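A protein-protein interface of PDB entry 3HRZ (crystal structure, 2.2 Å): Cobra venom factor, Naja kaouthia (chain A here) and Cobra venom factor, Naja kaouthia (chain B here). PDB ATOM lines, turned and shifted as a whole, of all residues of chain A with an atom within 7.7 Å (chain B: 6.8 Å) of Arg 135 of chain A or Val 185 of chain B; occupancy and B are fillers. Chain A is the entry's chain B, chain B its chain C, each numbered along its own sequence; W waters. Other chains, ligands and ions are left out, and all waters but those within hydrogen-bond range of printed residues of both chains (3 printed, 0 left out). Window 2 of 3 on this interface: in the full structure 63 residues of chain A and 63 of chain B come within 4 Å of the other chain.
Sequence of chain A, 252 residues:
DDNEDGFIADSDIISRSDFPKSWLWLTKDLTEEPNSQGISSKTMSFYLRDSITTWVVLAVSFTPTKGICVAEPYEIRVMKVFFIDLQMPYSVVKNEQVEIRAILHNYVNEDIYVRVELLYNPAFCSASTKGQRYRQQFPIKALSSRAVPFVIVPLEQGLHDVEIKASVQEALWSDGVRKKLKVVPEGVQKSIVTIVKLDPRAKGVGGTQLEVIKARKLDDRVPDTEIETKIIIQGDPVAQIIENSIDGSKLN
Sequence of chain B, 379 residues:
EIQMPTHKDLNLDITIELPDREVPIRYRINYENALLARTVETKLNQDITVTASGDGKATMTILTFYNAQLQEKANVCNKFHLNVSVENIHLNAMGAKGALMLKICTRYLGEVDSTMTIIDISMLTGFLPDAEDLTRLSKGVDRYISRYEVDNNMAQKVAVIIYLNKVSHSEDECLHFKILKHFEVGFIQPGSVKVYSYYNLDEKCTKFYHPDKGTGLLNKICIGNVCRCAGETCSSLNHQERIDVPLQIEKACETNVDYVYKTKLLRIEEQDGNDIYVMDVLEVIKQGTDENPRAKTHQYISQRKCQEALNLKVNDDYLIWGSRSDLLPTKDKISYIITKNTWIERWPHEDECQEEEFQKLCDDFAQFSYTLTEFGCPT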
ATOM      1  N   ASP A   5      23.563  -0.283  -3.427  1.00  0.00           N
ATOM      2  CA  ASP A   5      23.346   0.694  -4.502  1.00  0.00           C
ATOM      3  C   ASP A   5      22.196   1.659  -4.193  1.00  0.00           C
ATOM      4  O   ASP A   5      21.047   1.436  -4.582  1.00  0.00           O
ATOM      5  CB  ASP A   5      23.104   0.001  -5.846  1.00  0.00           C
ATOM      6  CG  ASP A   5      21.961  -1.001  -5.795  1.00  0.00           C
ATOM      7  OD1 ASP A   5      22.218  -2.175  -5.446  1.00  0.00           O
ATOM      8  OD2 ASP A   5      20.811  -0.624  -6.117  1.00  0.00           O
ATOM      9  N   PHE A   7      21.684   2.084  -1.162  1.00  0.00           N
ATOM     10  CA  PHE A   7      21.442   1.597   0.187  1.00  0.00           C
ATOM     11  C   PHE A   7      22.614   1.859   1.122  1.00  0.00           C
ATOM     12  O   PHE A   7      23.757   1.991   0.689  1.00  0.00           O
ATOM     13  CB  PHE A   7      21.131   0.104   0.177  1.00  0.00           C
ATOM     14  CG  PHE A   7      19.835  -0.240  -0.502  1.00  0.00           C
ATOM     15  CD1 PHE A   7      18.633  -0.113   0.168  1.00  0.00           C
ATOM     16  CD2 PHE A   7      19.821  -0.700  -1.806  1.00  0.00           C
ATOM     17  CE1 PHE A   7      17.447  -0.433  -0.450  1.00  0.00           C
ATOM     18  CE2 PHE A   7      18.632  -1.023  -2.429  1.00  0.00           C
ATOM     19  CZ  PHE A   7      17.446  -0.889  -1.751  1.00  0.00           C
ATOM     20  N   ILE A   8      22.307   1.925   2.413  1.00  0.00           N
ATOM     21  CA  ILE A   8      23.320   2.016   3.453  1.00  0.00           C
ATOM     22  C   ILE A   8      24.265   0.817   3.390  1.00  0.00           C
ATOM     23  O   ILE A   8      23.818  -0.323   3.245  1.00  0.00           O
ATOM     24  CB  ILE A   8      22.664   2.043   4.855  1.00  0.00           C
ATOM     25  CG1 ILE A   8      21.700   3.222   4.975  1.00  0.00           C
ATOM     26  CG2 ILE A   8      23.710   2.134   5.936  1.00  0.00           C
ATOM     27  CD1 ILE A   8      22.356   4.572   4.747  1.00  0.00           C
ATOM     28  N   ASP A  10      26.354  -2.138   4.772  1.00  0.00           N
ATOM     29  CA  ASP A  10      26.061  -3.023   5.893  1.00  0.00           C
ATOM     30  C   ASP A  10      26.852  -2.689   7.157  1.00  0.00           C
ATOM     31  O   ASP A  10      26.300  -2.708   8.258  1.00  0.00           O
ATOM     32  CB  ASP A  10      26.324  -4.482   5.536  1.00  0.00           C
ATOM     33  CG  ASP A  10      26.017  -5.415   6.695  1.00  0.00           C
ATOM     34  OD1 ASP A  10      24.820  -5.579   7.012  1.00  0.00           O
ATOM     35  OD2 ASP A  10      26.963  -5.972   7.299  1.00  0.00           O
ATOM     36  N   VAL A 114      13.033  -0.716   0.206  1.00  0.00           N
ATOM     37  CA  VAL A 114      13.927  -1.219   1.233  1.00  0.00           C
ATOM     38  C   VAL A 114      14.655  -2.489   0.835  1.00  0.00           C
ATOM     39  O   VAL A 114      14.210  -3.241  -0.042  1.00  0.00           O
ATOM     40  CB  VAL A 114      13.173  -1.515   2.535  1.00  0.00           C
ATOM     41  CG1 VAL A 114      12.305  -0.326   2.916  1.00  0.00           C
ATOM     42  CG2 VAL A 114      12.322  -2.759   2.360  1.00  0.00           C
ATOM     43  N   ARG A 115      15.778  -2.706   1.513  1.00  0.00           N
ATOM     44  CA  ARG A 115      16.571  -3.919   1.396  1.00  0.00           C
ATOM     45  C   ARG A 115      16.619  -4.583   2.756  1.00  0.00           C
ATOM     46  O   ARG A 115      16.883  -3.924   3.773  1.00  0.00           O
ATOM     47  CB  ARG A 115      17.988  -3.589   0.933  1.00  0.00           C
ATOM     48  CG  ARG A 115      18.960  -4.748   1.091  1.00  0.00           C
ATOM     49  CD  ARG A 115      20.360  -4.386   0.630  1.00  0.00           C
ATOM     50  NE  ARG A 115      20.427  -4.161  -0.811  1.00  0.00           N
ATOM     51  CZ  ARG A 115      21.491  -3.657  -1.433  1.00  0.00           C
ATOM     52  NH1 ARG A 115      22.571  -3.314  -0.741  1.00  0.00           N
ATOM     53  NH2 ARG A 115      21.472  -3.479  -2.745  1.00  0.00           N
ATOM     54  N   VAL A 116      16.349  -5.882   2.783  1.00  0.00           N
ATOM     55  CA  VAL A 116      16.357  -6.649   4.029  1.00  0.00           C
ATOM     56  C   VAL A 116      17.221  -7.876   3.822  1.00  0.00           C
ATOM     57  O   VAL A 116      17.128  -8.526   2.778  1.00  0.00           O
ATOM     58  CB  VAL A 116      14.964  -7.154   4.400  1.00  0.00           C
ATOM     59  CG1 VAL A 116      14.962  -7.627   5.839  1.00  0.00           C
ATOM     60  CG2 VAL A 116      13.939  -6.075   4.184  1.00  0.00           C
ATOM     61  N   GLU A 117      18.047  -8.199   4.814  1.00  0.00           N
ATOM     62  CA  GLU A 117      18.952  -9.347   4.722  1.00  0.00           C
ATOM     63  C   GLU A 117      18.919 -10.186   5.995  1.00  0.00           C
ATOM     64  O   GLU A 117      18.850  -9.646   7.102  1.00  0.00           O
ATOM     65  CB  GLU A 117      20.395  -8.889   4.451  1.00  0.00           C
ATOM     66  CG  GLU A 117      20.650  -8.394   3.031  1.00  0.00           C
ATOM     67  CD  GLU A 117      22.090  -7.939   2.819  1.00  0.00           C
ATOM     68  OE1 GLU A 117      22.744  -7.567   3.817  1.00  0.00           O
ATOM     69  OE2 GLU A 117      22.570  -7.953   1.661  1.00  0.00           O
ATOM     70  N   LEU A 118      18.963 -11.504   5.835  1.00  0.00           N
ATOM     71  CA  LEU A 118      19.108 -12.387   6.978  1.00  0.00           C
ATOM     72  C   LEU A 118      20.560 -12.797   7.036  1.00  0.00           C
ATOM     73  O   LEU A 118      21.123 -13.213   6.027  1.00  0.00           O
ATOM     74  CB  LEU A 118      18.224 -13.612   6.822  1.00  0.00           C
ATOM     75  CG  LEU A 118      18.450 -14.718   7.848  1.00  0.00           C
ATOM     76  CD1 LEU A 118      17.858 -14.312   9.185  1.00  0.00           C
ATOM     77  CD2 LEU A 118      17.844 -16.043   7.346  1.00  0.00           C
ATOM     78  N   ALA A 127      18.048 -19.626   4.089  1.00  0.00           N
ATOM     79  CA  ALA A 127      18.339 -19.230   2.715  1.00  0.00           C
ATOM     80  C   ALA A 127      19.709 -18.560   2.592  1.00  0.00           C
ATOM     81  O   ALA A 127      20.256 -18.457   1.504  1.00  0.00           O
ATOM     82  CB  ALA A 127      17.262 -18.322   2.193  1.00  0.00           C
ATOM     83  N   SER A 128      20.252 -18.089   3.710  1.00  0.00           N
ATOM     84  CA  SER A 128      21.589 -17.500   3.715  1.00  0.00           C
ATOM     85  C   SER A 128      22.687 -18.554   3.727  1.00  0.00           C
ATOM     86  O   SER A 128      22.535 -19.636   4.304  1.00  0.00           O
ATOM     87  CB  SER A 128      21.770 -16.576   4.918  1.00  0.00           C
ATOM     88  OG  SER A 128      21.062 -15.373   4.716  1.00  0.00           O
ATOM     89  N   GLN A 132      27.000 -15.884   0.792  1.00  0.00           N
ATOM     90  CA  GLN A 132      25.955 -15.016   0.267  1.00  0.00           C
ATOM     91  C   GLN A 132      24.791 -14.820   1.236  1.00  0.00           C
ATOM     92  O   GLN A 132      24.085 -15.771   1.569  1.00  0.00           O
ATOM     93  CB  GLN A 132      25.431 -15.610  -1.043  1.00  0.00           C
ATOM     94  CG  GLN A 132      24.305 -14.833  -1.684  1.00  0.00           C
ATOM     95  CD  GLN A 132      24.791 -13.563  -2.341  1.00  0.00           C
ATOM     96  OE1 GLN A 132      25.417 -12.719  -1.696  1.00  0.00           O
ATOM     97  NE2 GLN A 132      24.510 -13.417  -3.635  1.00  0.00           N
ATOM     98  N   ARG A 133      24.584 -13.584   1.679  1.00  0.00           N
ATOM     99  CA  ARG A 133      23.417 -13.275   2.497  1.00  0.00           C
ATOM    100  C   ARG A 133      22.138 -13.299   1.686  1.00  0.00           C
ATOM    101  O   ARG A 133      22.094 -12.870   0.534  1.00  0.00           O
ATOM    102  CB  ARG A 133      23.550 -11.918   3.187  1.00  0.00           C
ATOM    103  CG  ARG A 133      24.281 -11.977   4.497  1.00  0.00           C
ATOM    104  CD  ARG A 133      24.338 -10.609   5.108  1.00  0.00           C
ATOM    105  NE  ARG A 133      25.460 -10.474   6.025  1.00  0.00           N
ATOM    106  CZ  ARG A 133      25.791  -9.330   6.607  1.00  0.00           C
ATOM    107  NH1 ARG A 133      25.077  -8.242   6.355  1.00  0.00           N
ATOM    108  NH2 ARG A 133      26.827  -9.270   7.432  1.00  0.00           N
ATOM    109  N   TYR A 134      21.084 -13.799   2.306  1.00  0.00           N
ATOM    110  CA  TYR A 134      19.804 -13.805   1.659  1.00  0.00           C
ATOM    111  C   TYR A 134      19.225 -12.389   1.669  1.00  0.00           C
ATOM    112  O   TYR A 134      18.932 -11.834   2.728  1.00  0.00           O
ATOM    113  CB  TYR A 134      18.871 -14.780   2.358  1.00  0.00           C
ATOM    114  CG  TYR A 134      17.578 -14.909   1.621  1.00  0.00           C
ATOM    115  CD1 TYR A 134      17.556 -15.414   0.320  1.00  0.00           C
ATOM    116  CD2 TYR A 134      16.380 -14.505   2.198  1.00  0.00           C
ATOM    117  CE1 TYR A 134      16.371 -15.522  -0.380  1.00  0.00           C
ATOM    118  CE2 TYR A 134      15.188 -14.613   1.507  1.00  0.00           C
ATOM    119  CZ  TYR A 134      15.188 -15.121   0.220  1.00  0.00           C
ATOM    120  OH  TYR A 134      14.008 -15.235  -0.475  1.00  0.00           O
ATOM    121  N   ARG A 135      19.065 -11.809   0.482  1.00  0.00           N
ATOM    122  CA  ARG A 135      18.672 -10.408   0.352  1.00  0.00           C
ATOM    123  C   ARG A 135      17.360 -10.232  -0.422  1.00  0.00           C
ATOM    124  O   ARG A 135      17.177 -10.860  -1.458  1.00  0.00           O
ATOM    125  CB  ARG A 135      19.793  -9.650  -0.361  1.00  0.00           C
ATOM    126  CG  ARG A 135      19.487  -8.199  -0.648  1.00  0.00           C
ATOM    127  CD  ARG A 135      20.571  -7.577  -1.515  1.00  0.00           C
ATOM    128  NE  ARG A 135      21.846  -7.501  -0.810  1.00  0.00           N
ATOM    129  CZ  ARG A 135      22.930  -6.894  -1.285  1.00  0.00           C
ATOM    130  NH1 ARG A 135      22.897  -6.312  -2.475  1.00  0.00           N
ATOM    131  NH2 ARG A 135      24.047  -6.865  -0.567  1.00  0.00           N
ATOM    132  N   GLN A 136      16.454  -9.386   0.074  1.00  0.00           N
ATOM    133  CA  GLN A 136      15.269  -8.997  -0.700  1.00  0.00           C
ATOM    134  C   GLN A 136      15.138  -7.487  -0.781  1.00  0.00           C
ATOM    135  O   GLN A 136      15.608  -6.759   0.094  1.00  0.00           O
ATOM    136  CB  GLN A 136      13.978  -9.540  -0.095  1.00  0.00           C
ATOM    137  CG  GLN A 136      14.129 -10.751   0.768  1.00  0.00           C
ATOM    138  CD  GLN A 136      12.915 -10.964   1.633  1.00  0.00           C
ATOM    139  OE1 GLN A 136      12.992 -11.551   2.722  1.00  0.00           O
ATOM    140  NE2 GLN A 136      11.781 -10.479   1.161  1.00  0.00           N
ATOM    141  N   GLN A 137      14.466  -7.021  -1.826  1.00  0.00           N
ATOM    142  CA  GLN A 137      14.166  -5.611  -1.968  1.00  0.00           C
ATOM    143  C   GLN A 137      12.709  -5.427  -2.398  1.00  0.00           C
ATOM    144  O   GLN A 137      12.211  -6.130  -3.280  1.00  0.00           O
ATOM    145  CB  GLN A 137      15.143  -4.959  -2.949  1.00  0.00           C
ATOM    146  CG  GLN A 137      16.594  -5.090  -2.490  1.00  0.00           C
ATOM    147  CD  GLN A 137      17.597  -4.534  -3.482  1.00  0.00           C
ATOM    148  OE1 GLN A 137      18.802  -4.586  -3.247  1.00  0.00           O
ATOM    149  NE2 GLN A 137      17.107  -4.006  -4.599  1.00  0.00           N
ATOM    150  N   PHE A 138      12.022  -4.497  -1.749  1.00  0.00           N
ATOM    151  CA  PHE A 138      10.607  -4.292  -2.006  1.00  0.00           C
ATOM    152  C   PHE A 138      10.173  -2.953  -1.453  1.00  0.00           C
ATOM    153  O   PHE A 138      10.799  -2.444  -0.541  1.00  0.00           O
ATOM    154  CB  PHE A 138       9.783  -5.416  -1.374  1.00  0.00           C
ATOM    155  CG  PHE A 138      10.075  -5.647   0.085  1.00  0.00           C
ATOM    156  CD1 PHE A 138       9.479  -4.868   1.061  1.00  0.00           C
ATOM    157  CD2 PHE A 138      10.929  -6.658   0.483  1.00  0.00           C
ATOM    158  CE1 PHE A 138       9.752  -5.086   2.407  1.00  0.00           C
ATOM    159  CE2 PHE A 138      11.200  -6.878   1.831  1.00  0.00           C
ATOM    160  CZ  PHE A 138      10.610  -6.096   2.789  1.00  0.00           C
ATOM    161  N   PHE A 150      11.027 -15.426   7.657  1.00  0.00           N
ATOM    162  CA  PHE A 150      12.294 -16.092   7.410  1.00  0.00           C
ATOM    163  C   PHE A 150      12.162 -17.525   7.837  1.00  0.00           C
ATOM    164  O   PHE A 150      11.673 -17.805   8.931  1.00  0.00           O
ATOM    165  CB  PHE A 150      13.427 -15.388   8.147  1.00  0.00           C
ATOM    166  CG  PHE A 150      13.737 -14.046   7.582  1.00  0.00           C
ATOM    167  CD1 PHE A 150      14.406 -13.937   6.369  1.00  0.00           C
ATOM    168  CD2 PHE A 150      13.322 -12.900   8.222  1.00  0.00           C
ATOM    169  CE1 PHE A 150      14.682 -12.694   5.822  1.00  0.00           C
ATOM    170  CE2 PHE A 150      13.598 -11.657   7.687  1.00  0.00           C
ATOM    171  CZ  PHE A 150      14.278 -11.553   6.486  1.00  0.00           C
ATOM    172  N   THR B 125       8.313 -15.971  -0.687  1.00  0.00           N
ATOM    173  CA  THR B 125       9.031 -14.721  -0.917  1.00  0.00           C
ATOM    174  C   THR B 125       8.672 -14.073  -2.251  1.00  0.00           C
ATOM    175  O   THR B 125       8.817 -14.681  -3.307  1.00  0.00           O
ATOM    176  CB  THR B 125      10.567 -14.921  -0.899  1.00  0.00           C
ATOM    177  OG1 THR B 125      10.938 -15.776   0.186  1.00  0.00           O
ATOM    178  CG2 THR B 125      11.266 -13.578  -0.729  1.00  0.00           C
ATOM    179  N   GLY B 126       8.220 -12.827  -2.201  1.00  0.00           N
ATOM    180  CA  GLY B 126       7.946 -12.072  -3.403  1.00  0.00           C
ATOM    181  C   GLY B 126       6.562 -12.304  -3.982  1.00  0.00           C
ATOM    182  O   GLY B 126       6.235 -11.764  -5.030  1.00  0.00           O
ATOM    183  N   PHE B 127       5.745 -13.107  -3.315  1.00  0.00           N
ATOM    184  CA  PHE B 127       4.388 -13.346  -3.795  1.00  0.00           C
ATOM    185  C   PHE B 127       3.360 -12.639  -2.926  1.00  0.00           C
ATOM    186  O   PHE B 127       3.588 -12.443  -1.724  1.00  0.00           O
ATOM    187  CB  PHE B 127       4.090 -14.843  -3.856  1.00  0.00           C
ATOM    188  CG  PHE B 127       4.700 -15.533  -5.046  1.00  0.00           C
ATOM    189  CD1 PHE B 127       3.910 -15.944  -6.111  1.00  0.00           C
ATOM    190  CD2 PHE B 127       6.059 -15.751  -5.109  1.00  0.00           C
ATOM    191  CE1 PHE B 127       4.475 -16.577  -7.216  1.00  0.00           C
ATOM    192  CE2 PHE B 127       6.633 -16.391  -6.207  1.00  0.00           C
ATOM    193  CZ  PHE B 127       5.834 -16.795  -7.262  1.00  0.00           C
ATOM    194  N   LYS B 181       3.200 -13.045  -8.459  1.00  0.00           N
ATOM    195  CA  LYS B 181       4.554 -12.565  -8.185  1.00  0.00           C
ATOM    196  C   LYS B 181       4.629 -11.041  -8.072  1.00  0.00           C
ATOM    197  O   LYS B 181       4.370 -10.310  -9.033  1.00  0.00           O
ATOM    198  CB  LYS B 181       5.552 -13.060  -9.242  1.00  0.00           C
ATOM    199  CG  LYS B 181       6.995 -12.636  -8.958  1.00  0.00           C
ATOM    200  CD  LYS B 181       8.004 -13.438  -9.777  1.00  0.00           C
ATOM    201  CE  LYS B 181       8.153 -14.855  -9.241  1.00  0.00           C
ATOM    202  NZ  LYS B 181       9.305 -15.602  -9.850  1.00  0.00           N
ATOM    203  N   PHE B 183       7.609  -9.374  -6.435  1.00  0.00           N
ATOM    204  CA  PHE B 183       9.004  -9.108  -6.808  1.00  0.00           C
ATOM    205  C   PHE B 183       9.828 -10.397  -6.933  1.00  0.00           C
ATOM    206  O   PHE B 183       9.471 -11.438  -6.366  1.00  0.00           O
ATOM    207  CB  PHE B 183       9.657  -8.125  -5.818  1.00  0.00           C
ATOM    208  CG  PHE B 183       9.643  -8.594  -4.370  1.00  0.00           C
ATOM    209  CD1 PHE B 183      10.693  -9.340  -3.858  1.00  0.00           C
ATOM    210  CD2 PHE B 183       8.593  -8.268  -3.526  1.00  0.00           C
ATOM    211  CE1 PHE B 183      10.694  -9.761  -2.536  1.00  0.00           C
ATOM    212  CE2 PHE B 183       8.585  -8.688  -2.195  1.00  0.00           C
ATOM    213  CZ  PHE B 183       9.637  -9.437  -1.701  1.00  0.00           C
ATOM    214  N   GLU B 184      10.928 -10.334  -7.673  1.00  0.00           N
ATOM    215  CA  GLU B 184      11.783 -11.515  -7.843  1.00  0.00           C
ATOM    216  C   GLU B 184      12.919 -11.618  -6.824  1.00  0.00           C
ATOM    217  O   GLU B 184      13.428 -10.608  -6.335  1.00  0.00           O
ATOM    218  CB  GLU B 184      12.326 -11.610  -9.276  1.00  0.00           C
ATOM    219  CG  GLU B 184      11.529 -12.579 -10.144  1.00  0.00           C
ATOM    220  CD  GLU B 184      11.595 -12.241 -11.620  1.00  0.00           C
ATOM    221  OE1 GLU B 184      12.680 -12.403 -12.228  1.00  0.00           O
ATOM    222  OE2 GLU B 184      10.550 -11.824 -12.173  1.00  0.00           O
ATOM    223  N   VAL B 185      13.288 -12.851  -6.495  1.00  0.00           N
ATOM    224  CA  VAL B 185      14.443 -13.110  -5.636  1.00  0.00           C
ATOM    225  C   VAL B 185      15.314 -14.213  -6.214  1.00  0.00           C
ATOM    226  O   VAL B 185      14.880 -14.973  -7.079  1.00  0.00           O
ATOM    227  CB  VAL B 185      14.033 -13.506  -4.191  1.00  0.00           C
ATOM    228  CG1 VAL B 185      14.006 -12.285  -3.284  1.00  0.00           C
ATOM    229  CG2 VAL B 185      12.705 -14.245  -4.189  1.00  0.00           C
ATOM    230  N   GLY B 186      16.548 -14.299  -5.734  1.00  0.00           N
ATOM    231  CA  GLY B 186      17.428 -15.380  -6.138  1.00  0.00           C
ATOM    232  C   GLY B 186      16.806 -16.733  -5.835  1.00  0.00           C
ATOM    233  O   GLY B 186      16.750 -17.615  -6.691  1.00  0.00           O
ATOM    234  N   PHE B 187      16.329 -16.890  -4.605  1.00  0.00           N
ATOM    235  CA  PHE B 187      15.719 -18.137  -4.174  1.00  0.00           C
ATOM    236  C   PHE B 187      14.418 -17.803  -3.446  1.00  0.00           C
ATOM    237  O   PHE B 187      14.343 -16.800  -2.754  1.00  0.00           O
ATOM    238  CB  PHE B 187      16.694 -18.931  -3.282  1.00  0.00           C
ATOM    239  CG  PHE B 187      16.029 -19.991  -2.437  1.00  0.00           C
ATOM    240  CD1 PHE B 187      15.719 -21.236  -2.971  1.00  0.00           C
ATOM    241  CD2 PHE B 187      15.703 -19.737  -1.103  1.00  0.00           C
ATOM    242  CE1 PHE B 187      15.095 -22.209  -2.185  1.00  0.00           C
ATOM    243  CE2 PHE B 187      15.086 -20.704  -0.319  1.00  0.00           C
ATOM    244  CZ  PHE B 187      14.776 -21.937  -0.856  1.00  0.00           C
ATOM    245  N   ILE B 188      13.392 -18.627  -3.639  1.00  0.00           N
ATOM    246  CA  ILE B 188      12.090 -18.408  -3.019  1.00  0.00           C
ATOM    247  C   ILE B 188      12.005 -19.233  -1.755  1.00  0.00           C
ATOM    248  O   ILE B 188      12.086 -20.458  -1.813  1.00  0.00           O
ATOM    249  CB  ILE B 188      10.922 -18.858  -3.921  1.00  0.00           C
ATOM    250  CG1 ILE B 188      11.105 -18.387  -5.372  1.00  0.00           C
ATOM    251  CG2 ILE B 188       9.584 -18.385  -3.350  1.00  0.00           C
ATOM    252  CD1 ILE B 188      10.904 -16.919  -5.593  1.00  0.00           C
ATOM    253  N   GLN B 189      11.847 -18.564  -0.617  1.00  0.00           N
ATOM    254  CA  GLN B 189      11.620 -19.257   0.645  1.00  0.00           C
ATOM    255  C   GLN B 189      10.227 -19.872   0.688  1.00  0.00           C
ATOM    256  O   GLN B 189       9.247 -19.231   0.307  1.00  0.00           O
ATOM    257  CB  GLN B 189      11.727 -18.299   1.832  1.00  0.00           C
ATOM    258  CG  GLN B 189      13.115 -17.908   2.251  1.00  0.00           C
ATOM    259  CD  GLN B 189      13.089 -16.974   3.452  1.00  0.00           C
ATOM    260  OE1 GLN B 189      12.650 -15.824   3.363  1.00  0.00           O
ATOM    261  NE2 GLN B 189      13.545 -17.468   4.580  1.00  0.00           N
HETATM  262  O   HOH W   1      10.581 -13.211   3.310  1.00  0.00           O
HETATM  263  O   HOH W   2      17.953 -13.485  -2.740  1.00  0.00           O
HETATM  264  O   HOH W   3      15.679 -18.783   5.230  1.00  0.00           O
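The side-chain hydroxyl (OH) of Tyr 134 of chain A sits at hydrogen-bond distance from the backbone carbonyl oxygen (O) of Phe 187 of chain B (2.8 Å).
The side-chain hydroxyl (OH) of Tyr 134 of chain A sits at hydrogen-bond distance from the side-chain hydroxyl (OG1) of Thr 125 of chain B (3.2 Å).
Water W3 bridges NE2 of Gln 189 of chain B (2.6 Å) and N of Ala 127 of chain A (2.8 Å).
Water W1 lies within hydrogen-bond range of OE1 of Gln 136 of chain A (3.0 Å) and OE1 of Gln 189 of chain B (3.3 Å).
Water W2 bridges the backbone carbonyl oxygen (O) of Arg 135 of chain A (3.0 Å) and the backbone NH (N) of Gly 186 of chain B (3.4 Å).
Printed residues of chain B within 4 Å of Arg 135 of chain A: Val 185.
Val 185 of chain B touches just one residue of chain A: Arg 135 (3.9 Å).
No residue of chain A comes within 4 Å of Gly 186 of chain B.
Of the printed residues of chain A, Thr 125 of chain B touches Tyr 134 (3.2 Å) and Gln 136 (3.7 Å).
Printed residues of chain B within 4 Å of Gln 137 of chain A: Phe 183.
The nearest residue of chain A that does not touch Val 185 of chain B is Tyr 134 of chain A (4.1 Å).
The side-chain carboxylate of Glu 117 of chain A lies within salt-bridge range of the guanidinium group of Arg 135 of chain A (2.6 Å).
The backbone carbonyl oxygen (O) of Val 116 of chain A lies within hydrogen-bond range of the backbone NH (N) of Gln 136 of chain A.
OG1 of Thr 125 of chain B lies within hydrogen-bond range of N of Gln 189 of chain B.
The backbone carbonyl oxygen of Tyr 134 of chain A is in hydrogen-bond range of the backbone NH of Leu 118 of chain A (3.1 Å).
O of Phe 138 of chain A is in hydrogen-bond range of N of Val 114 of chain A, at 2.9 Å.
O of Gly 126 of chain B sits at hydrogen-bond distance from N of Phe 183 of chain B (3.1 Å).
Hydrophobic or aromatic side chains of chain A within 4 Å of the printed part of chain B: Ala 127, Tyr 134, Phe 138 and Phe 150.
Of the 11 printed residues of chain B, 5 touch a printed residue of chain A.
Printed residues of chain B that touch a printed residue of chain A: Thr 125, Phe 183, Val 185, Phe 187 and Gln 189.
Hydrophobic or aromatic side chains of chain B that line the printed part of chain A: Phe 183, Val 185 and Phe 187.
Among the printed residues, 10 pairs touch across the chains.
Among the printed residues, no Asp or Glu carboxylate lies within 4 Å of a Lys or Arg side-chain nitrogen of the other chain.
Among the printed residues, merely in contact across the chains: Tyr 134 of chain A with Gln 189 of chain B (3.4 Å), Phe 150 of chain A with Gln 189 of chain B (3.4 Å), Phe 138 of chain A with Phe 183 of chain B (3.6 Å), Gln 137 of chain A with Phe 183 of chain B (3.6 Å), Gln 136 of chain A with Thr 125 of chain B (3.7 Å), Gln 136 of chain A with Phe 183 of chain B (3.7 Å), Ala 127 of chain A with Phe 187 of chain B (3.9 Å) and Arg 135 of chain A with Val 185 of chain B (3.9 Å).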
